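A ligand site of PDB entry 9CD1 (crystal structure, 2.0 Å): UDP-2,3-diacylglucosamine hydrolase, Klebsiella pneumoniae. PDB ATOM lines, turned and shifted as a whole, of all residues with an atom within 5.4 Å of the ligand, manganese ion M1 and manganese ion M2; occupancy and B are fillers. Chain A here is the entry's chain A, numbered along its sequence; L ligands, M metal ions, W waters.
The backbone NH (N) of Trp 46 is in hydrogen-bond range of an oxygen (O1) of the ligand (3.1 Å). NH1 of Arg 157 sits at hydrogen-bond distance from O2 of the ligand (2.8 Å). An oxygen (O3) of the ligand lies within hydrogen-bond range of the side-chain amide nitrogen (ND2) of Asn 79 (2.9 Å). An oxygen (O4) of the ligand is in hydrogen-bond range of the guanidinium group of Arg 80 (2.8 Å). The side-chain hydroxyl (OG) of Ser 160 sits at hydrogen-bond distance from a nitrogen (N4) of the ligand, at 2.9 Å.
OD2 of Asp 8 lies within hydrogen-bond range of N of His 195, at 2.7 Å. The side-chain hydroxyl (OG) of Ser 160 sits at hydrogen-bond distance from the backbone carbonyl oxygen (O) of Met 156 (3.4 Å). A ring nitrogen (ND1) of His 10 sits at hydrogen-bond distance from the side-chain carboxylate (OE1) of Glu 44, 2.8 Å away. The side-chain carboxylate of Asp 41 lies within hydrogen-bond range of the backbone NH of Arg 80 (3.1 Å). The backbone NH of Tyr 125 lies within hydrogen-bond range of the side-chain carboxylate of Asp 122 (3.0 Å). NH2 of Arg 80 lies within salt-bridge range of OE2 of Glu 44, 3.2 Å away. The backbone carbonyl oxygen (O) of Val 132 sits at hydrogen-bond distance from the side-chain amide nitrogen (NE2) of Gln 138 (2.8 Å).
CA of Ala 45 touches O1 of the ligand (3.1 Å). Phe 82 touches the ligand (CZ to N1, 3.8 Å). Leu 83 touches the ligand. Tyr 125 touches the ligand. Phe 128 touches the ligand (CD2 to C21, 3.4 Å). O of Val 132 touches CL1 of the ligand, at 3.6 Å. Ile 137 touches the ligand (CG2 to C24, 3.9 Å). Gln 138 touches the ligand. CD1 of Phe 141 touches C22 of the ligand (3.5 Å). Ile 152 touches the ligand (CG2 to F2, 3.5 Å). CB of Ala 153 touches O2 of the ligand, at 3.6 Å. Met 156 touches the ligand. Hydrophobic or aromatic side chains that line the ligand: Ala 45, Phe 82, Leu 83, Tyr 125, Phe 128, Ile 137, Phe 141, Ile 152, Ala 153, Met 156 and His 195. Within 4 Å of the ligand: Ala 45, Trp 46, Asn 79, Arg 80, Phe 82, Leu 83, Tyr 125, Phe 128, Val 132, Ile 137, Gln 138, Phe 141, Ile 152, Ala 153, Met 156, Arg 157, Ser 160 and His 195.
Within 4 Å of manganese ion M1: Asp 8, Asp 41, Asn 79, His 114 and His 195. Along chain A the residues within 4 Å of manganese ion M1 span positions 8 to 195.
Within 4 Å of manganese ion M2: Asp 8, His 10, Asp 41 and His 197. The nearest printed residue that does not touch manganese ion M2 is His 195 (4.2 Å).
Manganese ion M1 is bound by OD1 of Asn 79, water W1, OD2 of Asp 41, NE2 of His 114 and ND1 of His 195. Manganese ion M1 has five donor atoms within binding distance.
Manganese ion M2 is bound by water W1, 2.0 Å away. Manganese ion M2 is bound by OD1 of Asp 8 (2.0 Å). Manganese ion M2 is bound by a ring nitrogen (NE2) of His 10. Manganese ion M2 is bound by NE2 of His 197, 2.3 Å away. OD2 of Asp 41 is bound to manganese ion M2 (2.3 Å).
Water W2 lies within hydrogen-bond range of the side-chain amide nitrogen (ND2) of Asn 79 (3.0 Å) and an oxygen (O5) of the ligand (3.1 Å).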
ATOM      1  N   ASP A   8     -17.734  25.138  36.199  1.00  0.00           N
ATOM      2  CA  ASP A   8     -17.367  25.625  34.874  1.00  0.00           C
ATOM      3  C   ASP A   8     -16.271  24.774  34.236  1.00  0.00           C
ATOM      4  O   ASP A   8     -15.314  25.290  33.648  1.00  0.00           O
ATOM      5  CB  ASP A   8     -16.966  27.099  34.937  1.00  0.00           C
ATOM      6  CG  ASP A   8     -18.099  27.983  35.416  1.00  0.00           C
ATOM      7  OD1 ASP A   8     -19.099  28.113  34.683  1.00  0.00           O
ATOM      8  OD2 ASP A   8     -18.007  28.514  36.541  1.00  0.00           O
ATOM      9  N   HIS A  10     -17.139  22.581  31.829  1.00  0.00           N
ATOM     10  CA  HIS A  10     -17.608  22.551  30.443  1.00  0.00           C
ATOM     11  C   HIS A  10     -17.093  21.313  29.712  1.00  0.00           C
ATOM     12  O   HIS A  10     -16.541  21.388  28.609  1.00  0.00           O
ATOM     13  CB  HIS A  10     -17.194  23.834  29.696  1.00  0.00           C
ATOM     14  CG  HIS A  10     -17.806  25.082  30.265  1.00  0.00           C
ATOM     15  ND1 HIS A  10     -19.009  25.590  29.821  1.00  0.00           N
ATOM     16  CD2 HIS A  10     -17.381  25.914  31.236  1.00  0.00           C
ATOM     17  CE1 HIS A  10     -19.299  26.683  30.500  1.00  0.00           C
ATOM     18  NE2 HIS A  10     -18.320  26.905  31.368  1.00  0.00           N
ATOM     19  N   ASP A  41     -22.317  24.110  35.363  1.00  0.00           N
ATOM     20  CA  ASP A  41     -21.512  24.044  34.146  1.00  0.00           C
ATOM     21  C   ASP A  41     -20.464  22.933  34.226  1.00  0.00           C
ATOM     22  O   ASP A  41     -19.317  23.105  33.778  1.00  0.00           O
ATOM     23  CB  ASP A  41     -20.868  25.402  33.831  1.00  0.00           C
ATOM     24  CG  ASP A  41     -21.856  26.409  33.280  1.00  0.00           C
ATOM     25  OD1 ASP A  41     -23.068  26.085  33.210  1.00  0.00           O
ATOM     26  OD2 ASP A  41     -21.431  27.522  32.932  1.00  0.00           O
ATOM     27  N   GLU A  44     -20.561  21.024  29.045  1.00  0.00           N
ATOM     28  CA  GLU A  44     -20.775  22.097  28.090  1.00  0.00           C
ATOM     29  C   GLU A  44     -22.221  22.126  27.594  1.00  0.00           C
ATOM     30  O   GLU A  44     -22.733  23.193  27.221  1.00  0.00           O
ATOM     31  CB  GLU A  44     -19.802  21.960  26.912  1.00  0.00           C
ATOM     32  CG  GLU A  44     -20.052  22.898  25.735  1.00  0.00           C
ATOM     33  CD  GLU A  44     -19.850  24.369  26.061  1.00  0.00           C
ATOM     34  OE1 GLU A  44     -19.314  24.697  27.136  1.00  0.00           O
ATOM     35  OE2 GLU A  44     -20.244  25.217  25.227  1.00  0.00           O
ATOM     36  N   ALA A  45     -22.893  20.980  27.594  1.00  0.00           N
ATOM     37  CA  ALA A  45     -24.266  20.894  27.125  1.00  0.00           C
ATOM     38  C   ALA A  45     -24.959  19.715  27.789  1.00  0.00           C
ATOM     39  O   ALA A  45     -24.309  18.770  28.242  1.00  0.00           O
ATOM     40  CB  ALA A  45     -24.337  20.770  25.600  1.00  0.00           C
ATOM     41  N   TRP A  46     -26.290  19.781  27.826  1.00  0.00           N
ATOM     42  CA  TRP A  46     -27.098  18.678  28.344  1.00  0.00           C
ATOM     43  C   TRP A  46     -28.476  18.773  27.730  1.00  0.00           C
ATOM     44  O   TRP A  46     -29.103  19.833  27.782  1.00  0.00           O
ATOM     45  CB  TRP A  46     -27.190  18.713  29.876  1.00  0.00           C
ATOM     46  CG  TRP A  46     -27.541  17.385  30.487  1.00  0.00           C
ATOM     47  CD1 TRP A  46     -28.782  16.911  30.779  1.00  0.00           C
ATOM     48  CD2 TRP A  46     -26.613  16.363  30.890  1.00  0.00           C
ATOM     49  NE1 TRP A  46     -28.694  15.661  31.334  1.00  0.00           N
ATOM     50  CE2 TRP A  46     -27.379  15.298  31.419  1.00  0.00           C
ATOM     51  CE3 TRP A  46     -25.220  16.242  30.873  1.00  0.00           C
ATOM     52  CZ2 TRP A  46     -26.790  14.128  31.914  1.00  0.00           C
ATOM     53  CZ3 TRP A  46     -24.640  15.088  31.355  1.00  0.00           C
ATOM     54  CH2 TRP A  46     -25.428  14.044  31.871  1.00  0.00           C
ATOM     55  N   ILE A  47     -28.944  17.663  27.141  1.00  0.00           N
ATOM     56  CA  ILE A  47     -30.253  17.601  26.510  1.00  0.00           C
ATOM     57  C   ILE A  47     -31.155  16.555  27.155  1.00  0.00           C
ATOM     58  O   ILE A  47     -32.231  16.271  26.633  1.00  0.00           O
ATOM     59  CB  ILE A  47     -30.132  17.361  24.998  1.00  0.00           C
ATOM     60  CG1 ILE A  47     -29.392  16.046  24.716  1.00  0.00           C
ATOM     61  CG2 ILE A  47     -29.426  18.528  24.319  1.00  0.00           C
ATOM     62  CD1 ILE A  47     -29.557  15.544  23.298  1.00  0.00           C
ATOM     63  N   GLY A  78     -25.901  24.720  36.324  1.00  0.00           N
ATOM     64  CA  GLY A  78     -25.466  25.894  35.606  1.00  0.00           C
ATOM     65  C   GLY A  78     -26.394  26.218  34.444  1.00  0.00           C
ATOM     66  O   GLY A  78     -27.411  25.566  34.222  1.00  0.00           O
ATOM     67  N   ASN A  79     -26.024  27.257  33.702  1.00  0.00           N
ATOM     68  CA  ASN A  79     -26.818  27.625  32.535  1.00  0.00           C
ATOM     69  C   ASN A  79     -26.599  26.665  31.365  1.00  0.00           C
ATOM     70  O   ASN A  79     -27.457  26.602  30.473  1.00  0.00           O
ATOM     71  CB  ASN A  79     -26.508  29.049  32.094  1.00  0.00           C
ATOM     72  CG  ASN A  79     -25.035  29.276  31.820  1.00  0.00           C
ATOM     73  OD1 ASN A  79     -24.212  29.217  32.738  1.00  0.00           O
ATOM     74  ND2 ASN A  79     -24.698  29.525  30.560  1.00  0.00           N
ATOM     75  N   ARG A  80     -25.488  25.929  31.347  1.00  0.00           N
ATOM     76  CA  ARG A  80     -25.241  24.984  30.269  1.00  0.00           C
ATOM     77  C   ARG A  80     -25.922  23.639  30.525  1.00  0.00           C
ATOM     78  O   ARG A  80     -26.430  23.016  29.592  1.00  0.00           O
ATOM     79  CB  ARG A  80     -23.735  24.779  30.072  1.00  0.00           C
ATOM     80  CG  ARG A  80     -22.959  26.074  29.813  1.00  0.00           C
ATOM     81  CD  ARG A  80     -23.480  26.808  28.583  1.00  0.00           C
ATOM     82  NE  ARG A  80     -23.353  26.013  27.370  1.00  0.00           N
ATOM     83  CZ  ARG A  80     -23.526  26.489  26.141  1.00  0.00           C
ATOM     84  NH1 ARG A  80     -23.834  27.759  25.929  1.00  0.00           N
ATOM     85  NH2 ARG A  80     -23.374  25.672  25.101  1.00  0.00           N
ATOM     86  N   PHE A  82     -28.558  22.791  32.839  1.00  0.00           N
ATOM     87  CA  PHE A  82     -29.735  22.895  33.704  1.00  0.00           C
ATOM     88  C   PHE A  82     -30.668  21.696  33.576  1.00  0.00           C
ATOM     89  O   PHE A  82     -31.543  21.537  34.436  1.00  0.00           O
ATOM     90  CB  PHE A  82     -30.501  24.185  33.416  1.00  0.00           C
ATOM     91  CG  PHE A  82     -30.939  24.327  31.975  1.00  0.00           C
ATOM     92  CD1 PHE A  82     -30.100  24.909  31.036  1.00  0.00           C
ATOM     93  CD2 PHE A  82     -32.188  23.881  31.570  1.00  0.00           C
ATOM     94  CE1 PHE A  82     -30.497  25.045  29.723  1.00  0.00           C
ATOM     95  CE2 PHE A  82     -32.588  24.008  30.255  1.00  0.00           C
ATOM     96  CZ  PHE A  82     -31.743  24.586  29.324  1.00  0.00           C
ATOM     97  N   LEU A  83     -30.512  20.852  32.561  1.00  0.00           N
ATOM     98  CA  LEU A  83     -31.388  19.707  32.398  1.00  0.00           C
ATOM     99  C   LEU A  83     -30.866  18.437  33.064  1.00  0.00           C
ATOM    100  O   LEU A  83     -31.485  17.378  32.926  1.00  0.00           O
ATOM    101  CB  LEU A  83     -31.615  19.432  30.901  1.00  0.00           C
ATOM    102  CG  LEU A  83     -32.499  20.450  30.192  1.00  0.00           C
ATOM    103  CD1 LEU A  83     -32.719  20.069  28.736  1.00  0.00           C
ATOM    104  CD2 LEU A  83     -33.833  20.612  30.909  1.00  0.00           C
ATOM    105  N   HIS A 114     -24.573  28.971  41.224  1.00  0.00           N
ATOM    106  CA  HIS A 114     -23.775  29.016  39.996  1.00  0.00           C
ATOM    107  C   HIS A 114     -23.275  30.421  39.721  1.00  0.00           C
ATOM    108  O   HIS A 114     -22.138  30.607  39.274  1.00  0.00           O
ATOM    109  CB  HIS A 114     -24.589  28.498  38.811  1.00  0.00           C
ATOM    110  CG  HIS A 114     -23.820  28.489  37.528  1.00  0.00           C
ATOM    111  ND1 HIS A 114     -22.636  27.789  37.374  1.00  0.00           N
ATOM    112  CD2 HIS A 114     -24.039  29.108  36.345  1.00  0.00           C
ATOM    113  CE1 HIS A 114     -22.171  27.980  36.150  1.00  0.00           C
ATOM    114  NE2 HIS A 114     -23.005  28.777  35.504  1.00  0.00           N
ATOM    115  N   ASP A 116     -25.062  32.828  37.769  1.00  0.00           N
ATOM    116  CA  ASP A 116     -25.690  33.510  36.639  1.00  0.00           C
ATOM    117  C   ASP A 116     -26.874  34.365  37.078  1.00  0.00           C
ATOM    118  O   ASP A 116     -27.179  35.363  36.417  1.00  0.00           O
ATOM    119  CB  ASP A 116     -26.139  32.490  35.577  1.00  0.00           C
ATOM    120  CG  ASP A 116     -27.103  31.461  36.130  1.00  0.00           C
ATOM    121  OD1 ASP A 116     -26.770  30.810  37.140  1.00  0.00           O
ATOM    122  OD2 ASP A 116     -28.198  31.313  35.548  1.00  0.00           O
ATOM    123  N   ASP A 122     -27.897  41.555  32.329  1.00  0.00           N
ATOM    124  CA  ASP A 122     -28.069  40.858  31.044  1.00  0.00           C
ATOM    125  C   ASP A 122     -29.528  40.405  30.936  1.00  0.00           C
ATOM    126  O   ASP A 122     -29.883  39.264  31.216  1.00  0.00           O
ATOM    127  CB  ASP A 122     -27.092  39.690  30.938  1.00  0.00           C
ATOM    128  CG  ASP A 122     -26.958  39.170  29.519  1.00  0.00           C
ATOM    129  OD1 ASP A 122     -27.885  39.390  28.702  1.00  0.00           O
ATOM    130  OD2 ASP A 122     -25.922  38.548  29.208  1.00  0.00           O
ATOM    131  N   GLY A 124     -31.112  39.955  28.242  1.00  0.00           N
ATOM    132  CA  GLY A 124     -31.246  38.964  27.188  1.00  0.00           C
ATOM    133  C   GLY A 124     -31.043  37.550  27.688  1.00  0.00           C
ATOM    134  O   GLY A 124     -31.781  36.641  27.307  1.00  0.00           O
ATOM    135  N   TYR A 125     -30.040  37.340  28.546  1.00  0.00           N
ATOM    136  CA  TYR A 125     -29.843  36.012  29.103  1.00  0.00           C
ATOM    137  C   TYR A 125     -30.938  35.668  30.106  1.00  0.00           C
ATOM    138  O   TYR A 125     -31.399  34.518  30.169  1.00  0.00           O
ATOM    139  CB  TYR A 125     -28.476  35.896  29.783  1.00  0.00           C
ATOM    140  CG  TYR A 125     -28.414  34.688  30.690  1.00  0.00           C
ATOM    141  CD1 TYR A 125     -28.369  33.406  30.159  1.00  0.00           C
ATOM    142  CD2 TYR A 125     -28.459  34.836  32.073  1.00  0.00           C
ATOM    143  CE1 TYR A 125     -28.335  32.299  30.984  1.00  0.00           C
ATOM    144  CE2 TYR A 125     -28.423  33.738  32.901  1.00  0.00           C
ATOM    145  CZ  TYR A 125     -28.365  32.466  32.351  1.00  0.00           C
ATOM    146  OH  TYR A 125     -28.334  31.371  33.171  1.00  0.00           O
ATOM    147  N   PHE A 128     -33.854  34.255  28.406  1.00  0.00           N
ATOM    148  CA  PHE A 128     -33.569  32.859  28.068  1.00  0.00           C
ATOM    149  C   PHE A 128     -33.712  31.961  29.288  1.00  0.00           C
ATOM    150  O   PHE A 128     -34.344  30.900  29.228  1.00  0.00           O
ATOM    151  CB  PHE A 128     -32.168  32.748  27.468  1.00  0.00           C
ATOM    152  CG  PHE A 128     -31.712  31.330  27.241  1.00  0.00           C
ATOM    153  CD1 PHE A 128     -31.977  30.684  26.054  1.00  0.00           C
ATOM    154  CD2 PHE A 128     -30.998  30.651  28.223  1.00  0.00           C
ATOM    155  CE1 PHE A 128     -31.559  29.381  25.841  1.00  0.00           C
ATOM    156  CE2 PHE A 128     -30.574  29.344  28.018  1.00  0.00           C
ATOM    157  CZ  PHE A 128     -30.849  28.715  26.818  1.00  0.00           C
ATOM    158  N   LYS A 131     -37.259  31.212  30.312  1.00  0.00           N
ATOM    159  CA  LYS A 131     -37.939  30.296  29.410  1.00  0.00           C
ATOM    160  C   LYS A 131     -37.527  28.853  29.679  1.00  0.00           C
ATOM    161  O   LYS A 131     -38.387  27.989  29.941  1.00  0.00           O
ATOM    162  CB  LYS A 131     -37.649  30.682  27.965  1.00  0.00           C
ATOM    163  N   VAL A 132     -36.224  28.564  29.630  1.00  0.00           N
ATOM    164  CA  VAL A 132     -35.750  27.192  29.774  1.00  0.00           C
ATOM    165  C   VAL A 132     -35.895  26.650  31.183  1.00  0.00           C
ATOM    166  O   VAL A 132     -35.679  25.462  31.397  1.00  0.00           O
ATOM    167  CB  VAL A 132     -34.281  27.071  29.333  1.00  0.00           C
ATOM    168  CG1 VAL A 132     -34.127  27.420  27.858  1.00  0.00           C
ATOM    169  CG2 VAL A 132     -33.370  27.932  30.205  1.00  0.00           C
ATOM    170  N   ILE A 137     -42.042  23.994  29.577  1.00  0.00           N
ATOM    171  CA  ILE A 137     -41.096  24.086  28.470  1.00  0.00           C
ATOM    172  C   ILE A 137     -40.054  22.983  28.571  1.00  0.00           C
ATOM    173  O   ILE A 137     -39.675  22.367  27.564  1.00  0.00           O
ATOM    174  CB  ILE A 137     -40.451  25.484  28.428  1.00  0.00           C
ATOM    175  CG1 ILE A 137     -41.523  26.552  28.173  1.00  0.00           C
ATOM    176  CG2 ILE A 137     -39.360  25.552  27.371  1.00  0.00           C
ATOM    177  CD1 ILE A 137     -40.963  27.920  27.834  1.00  0.00           C
ATOM    178  N   GLN A 138     -39.568  22.710  29.794  1.00  0.00           N
ATOM    179  CA  GLN A 138     -38.601  21.625  29.975  1.00  0.00           C
ATOM    180  C   GLN A 138     -39.218  20.275  29.638  1.00  0.00           C
ATOM    181  O   GLN A 138     -38.590  19.447  28.974  1.00  0.00           O
ATOM    182  CB  GLN A 138     -38.081  21.618  31.412  1.00  0.00           C
ATOM    183  CG  GLN A 138     -37.208  22.799  31.768  1.00  0.00           C
ATOM    184  CD  GLN A 138     -36.476  22.591  33.083  1.00  0.00           C
ATOM    185  OE1 GLN A 138     -36.733  21.619  33.793  1.00  0.00           O
ATOM    186  NE2 GLN A 138     -35.573  23.513  33.407  1.00  0.00           N
ATOM    187  N   PHE A 141     -39.544  19.887  25.821  1.00  0.00           N
ATOM    188  CA  PHE A 141     -38.269  19.625  25.159  1.00  0.00           C
ATOM    189  C   PHE A 141     -37.791  18.198  25.410  1.00  0.00           C
ATOM    190  O   PHE A 141     -37.345  17.510  24.493  1.00  0.00           O
ATOM    191  CB  PHE A 141     -37.219  20.636  25.610  1.00  0.00           C
ATOM    192  CG  PHE A 141     -35.849  20.390  25.042  1.00  0.00           C
ATOM    193  CD1 PHE A 141     -35.522  20.814  23.774  1.00  0.00           C
ATOM    194  CD2 PHE A 141     -34.884  19.723  25.791  1.00  0.00           C
ATOM    195  CE1 PHE A 141     -34.262  20.583  23.245  1.00  0.00           C
ATOM    196  CE2 PHE A 141     -33.618  19.489  25.270  1.00  0.00           C
ATOM    197  CZ  PHE A 141     -33.310  19.921  23.993  1.00  0.00           C
ATOM    198  N   ARG A 149     -33.563  16.615  19.725  1.00  0.00           N
ATOM    199  CA  ARG A 149     -32.947  17.451  20.750  1.00  0.00           C
ATOM    200  C   ARG A 149     -31.498  17.773  20.415  1.00  0.00           C
ATOM    201  O   ARG A 149     -31.031  18.893  20.645  1.00  0.00           O
ATOM    202  CB  ARG A 149     -33.038  16.743  22.109  1.00  0.00           C
ATOM    203  CG  ARG A 149     -34.412  16.813  22.763  1.00  0.00           C
ATOM    204  CD  ARG A 149     -34.445  16.072  24.088  1.00  0.00           C
ATOM    205  NE  ARG A 149     -34.899  14.694  23.948  1.00  0.00           N
ATOM    206  CZ  ARG A 149     -34.534  13.704  24.741  1.00  0.00           C
ATOM    207  NH1 ARG A 149     -33.689  13.888  25.737  1.00  0.00           N
ATOM    208  NH2 ARG A 149     -35.036  12.483  24.533  1.00  0.00           N
ATOM    209  N   ILE A 152     -31.529  20.521  17.774  1.00  0.00           N
ATOM    210  CA  ILE A 152     -31.892  21.804  18.366  1.00  0.00           C
ATOM    211  C   ILE A 152     -30.707  22.386  19.139  1.00  0.00           C
ATOM    212  O   ILE A 152     -30.365  23.566  19.009  1.00  0.00           O
ATOM    213  CB  ILE A 152     -33.133  21.652  19.274  1.00  0.00           C
ATOM    214  CG1 ILE A 152     -34.364  21.306  18.455  1.00  0.00           C
ATOM    215  CG2 ILE A 152     -33.358  22.924  20.077  1.00  0.00           C
ATOM    216  CD1 ILE A 152     -35.554  20.908  19.293  1.00  0.00           C
ATOM    217  N   ALA A 153     -30.055  21.548  19.950  1.00  0.00           N
ATOM    218  CA  ALA A 153     -28.962  22.026  20.803  1.00  0.00           C
ATOM    219  C   ALA A 153     -27.774  22.489  19.968  1.00  0.00           C
ATOM    220  O   ALA A 153     -27.120  23.474  20.314  1.00  0.00           O
ATOM    221  CB  ALA A 153     -28.540  20.929  21.773  1.00  0.00           C
ATOM    222  N   MET A 156     -28.816  25.875  18.719  1.00  0.00           N
ATOM    223  CA  MET A 156     -28.991  26.854  19.783  1.00  0.00           C
ATOM    224  C   MET A 156     -27.661  27.275  20.396  1.00  0.00           C
ATOM    225  O   MET A 156     -27.512  28.422  20.821  1.00  0.00           O
ATOM    226  CB  MET A 156     -29.914  26.300  20.868  1.00  0.00           C
ATOM    227  CG  MET A 156     -31.382  26.487  20.568  1.00  0.00           C
ATOM    228  SD  MET A 156     -32.390  25.893  21.932  1.00  0.00           S
ATOM    229  CE  MET A 156     -31.665  26.798  23.292  1.00  0.00           C
ATOM    230  N   ARG A 157     -26.692  26.352  20.460  1.00  0.00           N
ATOM    231  CA  ARG A 157     -25.368  26.708  20.983  1.00  0.00           C
ATOM    232  C   ARG A 157     -24.726  27.802  20.132  1.00  0.00           C
ATOM    233  O   ARG A 157     -24.165  28.770  20.652  1.00  0.00           O
ATOM    234  CB  ARG A 157     -24.471  25.470  21.029  1.00  0.00           C
ATOM    235  CG  ARG A 157     -24.763  24.534  22.188  1.00  0.00           C
ATOM    236  CD  ARG A 157     -23.643  23.535  22.396  1.00  0.00           C
ATOM    237  NE  ARG A 157     -23.653  22.499  21.372  1.00  0.00           N
ATOM    238  CZ  ARG A 157     -24.424  21.420  21.399  1.00  0.00           C
ATOM    239  NH1 ARG A 157     -25.274  21.205  22.390  1.00  0.00           N
ATOM    240  NH2 ARG A 157     -24.357  20.535  20.409  1.00  0.00           N
ATOM    241  N   SER A 160     -26.740  31.146  20.884  1.00  0.00           N
ATOM    242  CA  SER A 160     -26.386  31.803  22.143  1.00  0.00           C
ATOM    243  C   SER A 160     -24.994  32.420  22.067  1.00  0.00           C
ATOM    244  O   SER A 160     -24.767  33.536  22.525  1.00  0.00           O
ATOM    245  CB  SER A 160     -26.448  30.795  23.305  1.00  0.00           C
ATOM    246  OG  SER A 160     -27.783  30.392  23.553  1.00  0.00           O
ATOM    247  N   ILE A 171     -19.050  36.401  28.517  1.00  0.00           N
ATOM    248  CA  ILE A 171     -19.944  36.338  29.664  1.00  0.00           C
ATOM    249  C   ILE A 171     -19.869  37.636  30.459  1.00  0.00           C
ATOM    250  O   ILE A 171     -18.792  38.060  30.867  1.00  0.00           O
ATOM    251  CB  ILE A 171     -19.625  35.138  30.561  1.00  0.00           C
ATOM    252  CG1 ILE A 171     -19.568  33.849  29.734  1.00  0.00           C
ATOM    253  CG2 ILE A 171     -20.651  35.006  31.673  1.00  0.00           C
ATOM    254  CD1 ILE A 171     -18.907  32.696  30.451  1.00  0.00           C
ATOM    255  N   HIS A 195     -19.588  30.651  37.004  1.00  0.00           N
ATOM    256  CA  HIS A 195     -20.270  31.228  35.843  1.00  0.00           C
ATOM    257  C   HIS A 195     -19.477  32.339  35.152  1.00  0.00           C
ATOM    258  O   HIS A 195     -19.371  32.344  33.924  1.00  0.00           O
ATOM    259  CB  HIS A 195     -21.652  31.762  36.226  1.00  0.00           C
ATOM    260  CG  HIS A 195     -22.374  32.401  35.084  1.00  0.00           C
ATOM    261  ND1 HIS A 195     -22.866  31.684  34.016  1.00  0.00           N
ATOM    262  CD2 HIS A 195     -22.670  33.700  34.821  1.00  0.00           C
ATOM    263  CE1 HIS A 195     -23.444  32.510  33.154  1.00  0.00           C
ATOM    264  NE2 HIS A 195     -23.331  33.735  33.616  1.00  0.00           N
ATOM    265  N   HIS A 197     -16.310  33.026  35.167  1.00  0.00           N
ATOM    266  CA  HIS A 197     -14.987  32.607  34.681  1.00  0.00           C
ATOM    267  C   HIS A 197     -13.913  33.627  35.050  1.00  0.00           C
ATOM    268  O   HIS A 197     -12.922  33.786  34.327  1.00  0.00           O
ATOM    269  CB  HIS A 197     -14.997  32.353  33.171  1.00  0.00           C
ATOM    270  CG  HIS A 197     -15.937  31.273  32.737  1.00  0.00           C
ATOM    271  ND1 HIS A 197     -15.978  30.791  31.446  1.00  0.00           N
ATOM    272  CD2 HIS A 197     -16.862  30.555  33.426  1.00  0.00           C
ATOM    273  CE1 HIS A 197     -16.890  29.847  31.348  1.00  0.00           C
ATOM    274  NE2 HIS A 197     -17.442  29.678  32.543  1.00  0.00           N
HETATM  275  C1  LIG L   1     -31.320  22.325  26.274  1.00  0.00           C
HETATM  276  C2  LIG L   1     -27.450  25.572  26.996  1.00  0.00           C
HETATM  277  C3  LIG L   1     -27.370  27.813  26.090  1.00  0.00           C
HETATM  278  C4  LIG L   1     -27.008  30.103  27.388  1.00  0.00           C
HETATM  279  C5  LIG L   1     -26.132  32.567  27.414  1.00  0.00           C
HETATM  280  C6  LIG L   1     -24.471  32.494  29.367  1.00  0.00           C
HETATM  281  C7  LIG L   1     -35.267  23.695  26.730  1.00  0.00           C
HETATM  282  C8  LIG L   1     -33.414  23.477  25.390  1.00  0.00           C
HETATM  283  C9  LIG L   1     -31.298  23.000  23.983  1.00  0.00           C
HETATM  284  C10 LIG L   1     -29.872  23.525  24.149  1.00  0.00           C
HETATM  285  C11 LIG L   1     -29.907  22.881  26.465  1.00  0.00           C
HETATM  286  C12 LIG L   1     -27.415  25.070  25.690  1.00  0.00           C
HETATM  287  C13 LIG L   1     -27.429  26.964  27.199  1.00  0.00           C
HETATM  288  C14 LIG L   1     -27.363  27.295  24.800  1.00  0.00           C
HETATM  289  C15 LIG L   1     -27.371  25.921  24.593  1.00  0.00           C
HETATM  290  C16 LIG L   1     -27.154  31.637  27.153  1.00  0.00           C
HETATM  291  C17 LIG L   1     -22.594  32.498  26.124  1.00  0.00           C
HETATM  292  C18 LIG L   1     -26.365  33.920  27.153  1.00  0.00           C
HETATM  293  C19 LIG L   1     -27.589  34.346  26.621  1.00  0.00           C
HETATM  294  C20 LIG L   1     -28.594  33.423  26.349  1.00  0.00           C
HETATM  295  C21 LIG L   1     -28.360  32.070  26.610  1.00  0.00           C
HETATM  296  C22 LIG L   1     -34.134  23.950  24.279  1.00  0.00           C
HETATM  297  C23 LIG L   1     -35.480  24.293  24.440  1.00  0.00           C
HETATM  298  C24 LIG L   1     -36.067  24.166  25.696  1.00  0.00           C
HETATM  299  C25 LIG L   1     -36.286  24.822  23.234  1.00  0.00           C
HETATM  300  F1  LIG L   1     -37.607  24.591  23.455  1.00  0.00           F
HETATM  301  F2  LIG L   1     -35.895  24.166  22.092  1.00  0.00           F
HETATM  302  F3  LIG L   1     -36.062  26.161  23.079  1.00  0.00           F
HETATM  303  N1  LIG L   1     -33.990  23.366  26.549  1.00  0.00           N
HETATM  304  N2  LIG L   1     -31.994  23.094  25.261  1.00  0.00           N
HETATM  305  N3  LIG L   1     -29.135  22.871  25.232  1.00  0.00           N
HETATM  306  N4  LIG L   1     -27.377  29.305  26.213  1.00  0.00           N
HETATM  307  N5  LIG L   1     -24.823  32.153  27.967  1.00  0.00           N
HETATM  308  O1  LIG L   1     -26.845  22.485  26.455  1.00  0.00           O
HETATM  309  O2  LIG L   1     -26.720  22.883  24.160  1.00  0.00           O
HETATM  310  O3  LIG L   1     -26.643  29.620  28.409  1.00  0.00           O
HETATM  311  O4  LIG L   1     -24.393  30.465  25.966  1.00  0.00           O
HETATM  312  O5  LIG L   1     -22.933  30.304  27.713  1.00  0.00           O
HETATM  313  S1  LIG L   1     -27.460  23.261  25.371  1.00  0.00           S
HETATM  314  S2  LIG L   1     -23.699  31.306  26.958  1.00  0.00           S
HETATM  315 CL1  LIG L   1     -35.950  23.498  28.366  1.00  0.00          CL
HETATM  316 MN    MN M   1     -22.384  29.421  33.443  1.00  0.00          MN
HETATM  317 MN    MN M   2     -19.299  28.365  32.713  1.00  0.00          MN
HETATM  318  O   HOH W   1     -20.515  29.912  32.583  1.00  0.00           O
HETATM  319  O   HOH W   2     -21.677  29.677  30.491  1.00  0.00           O
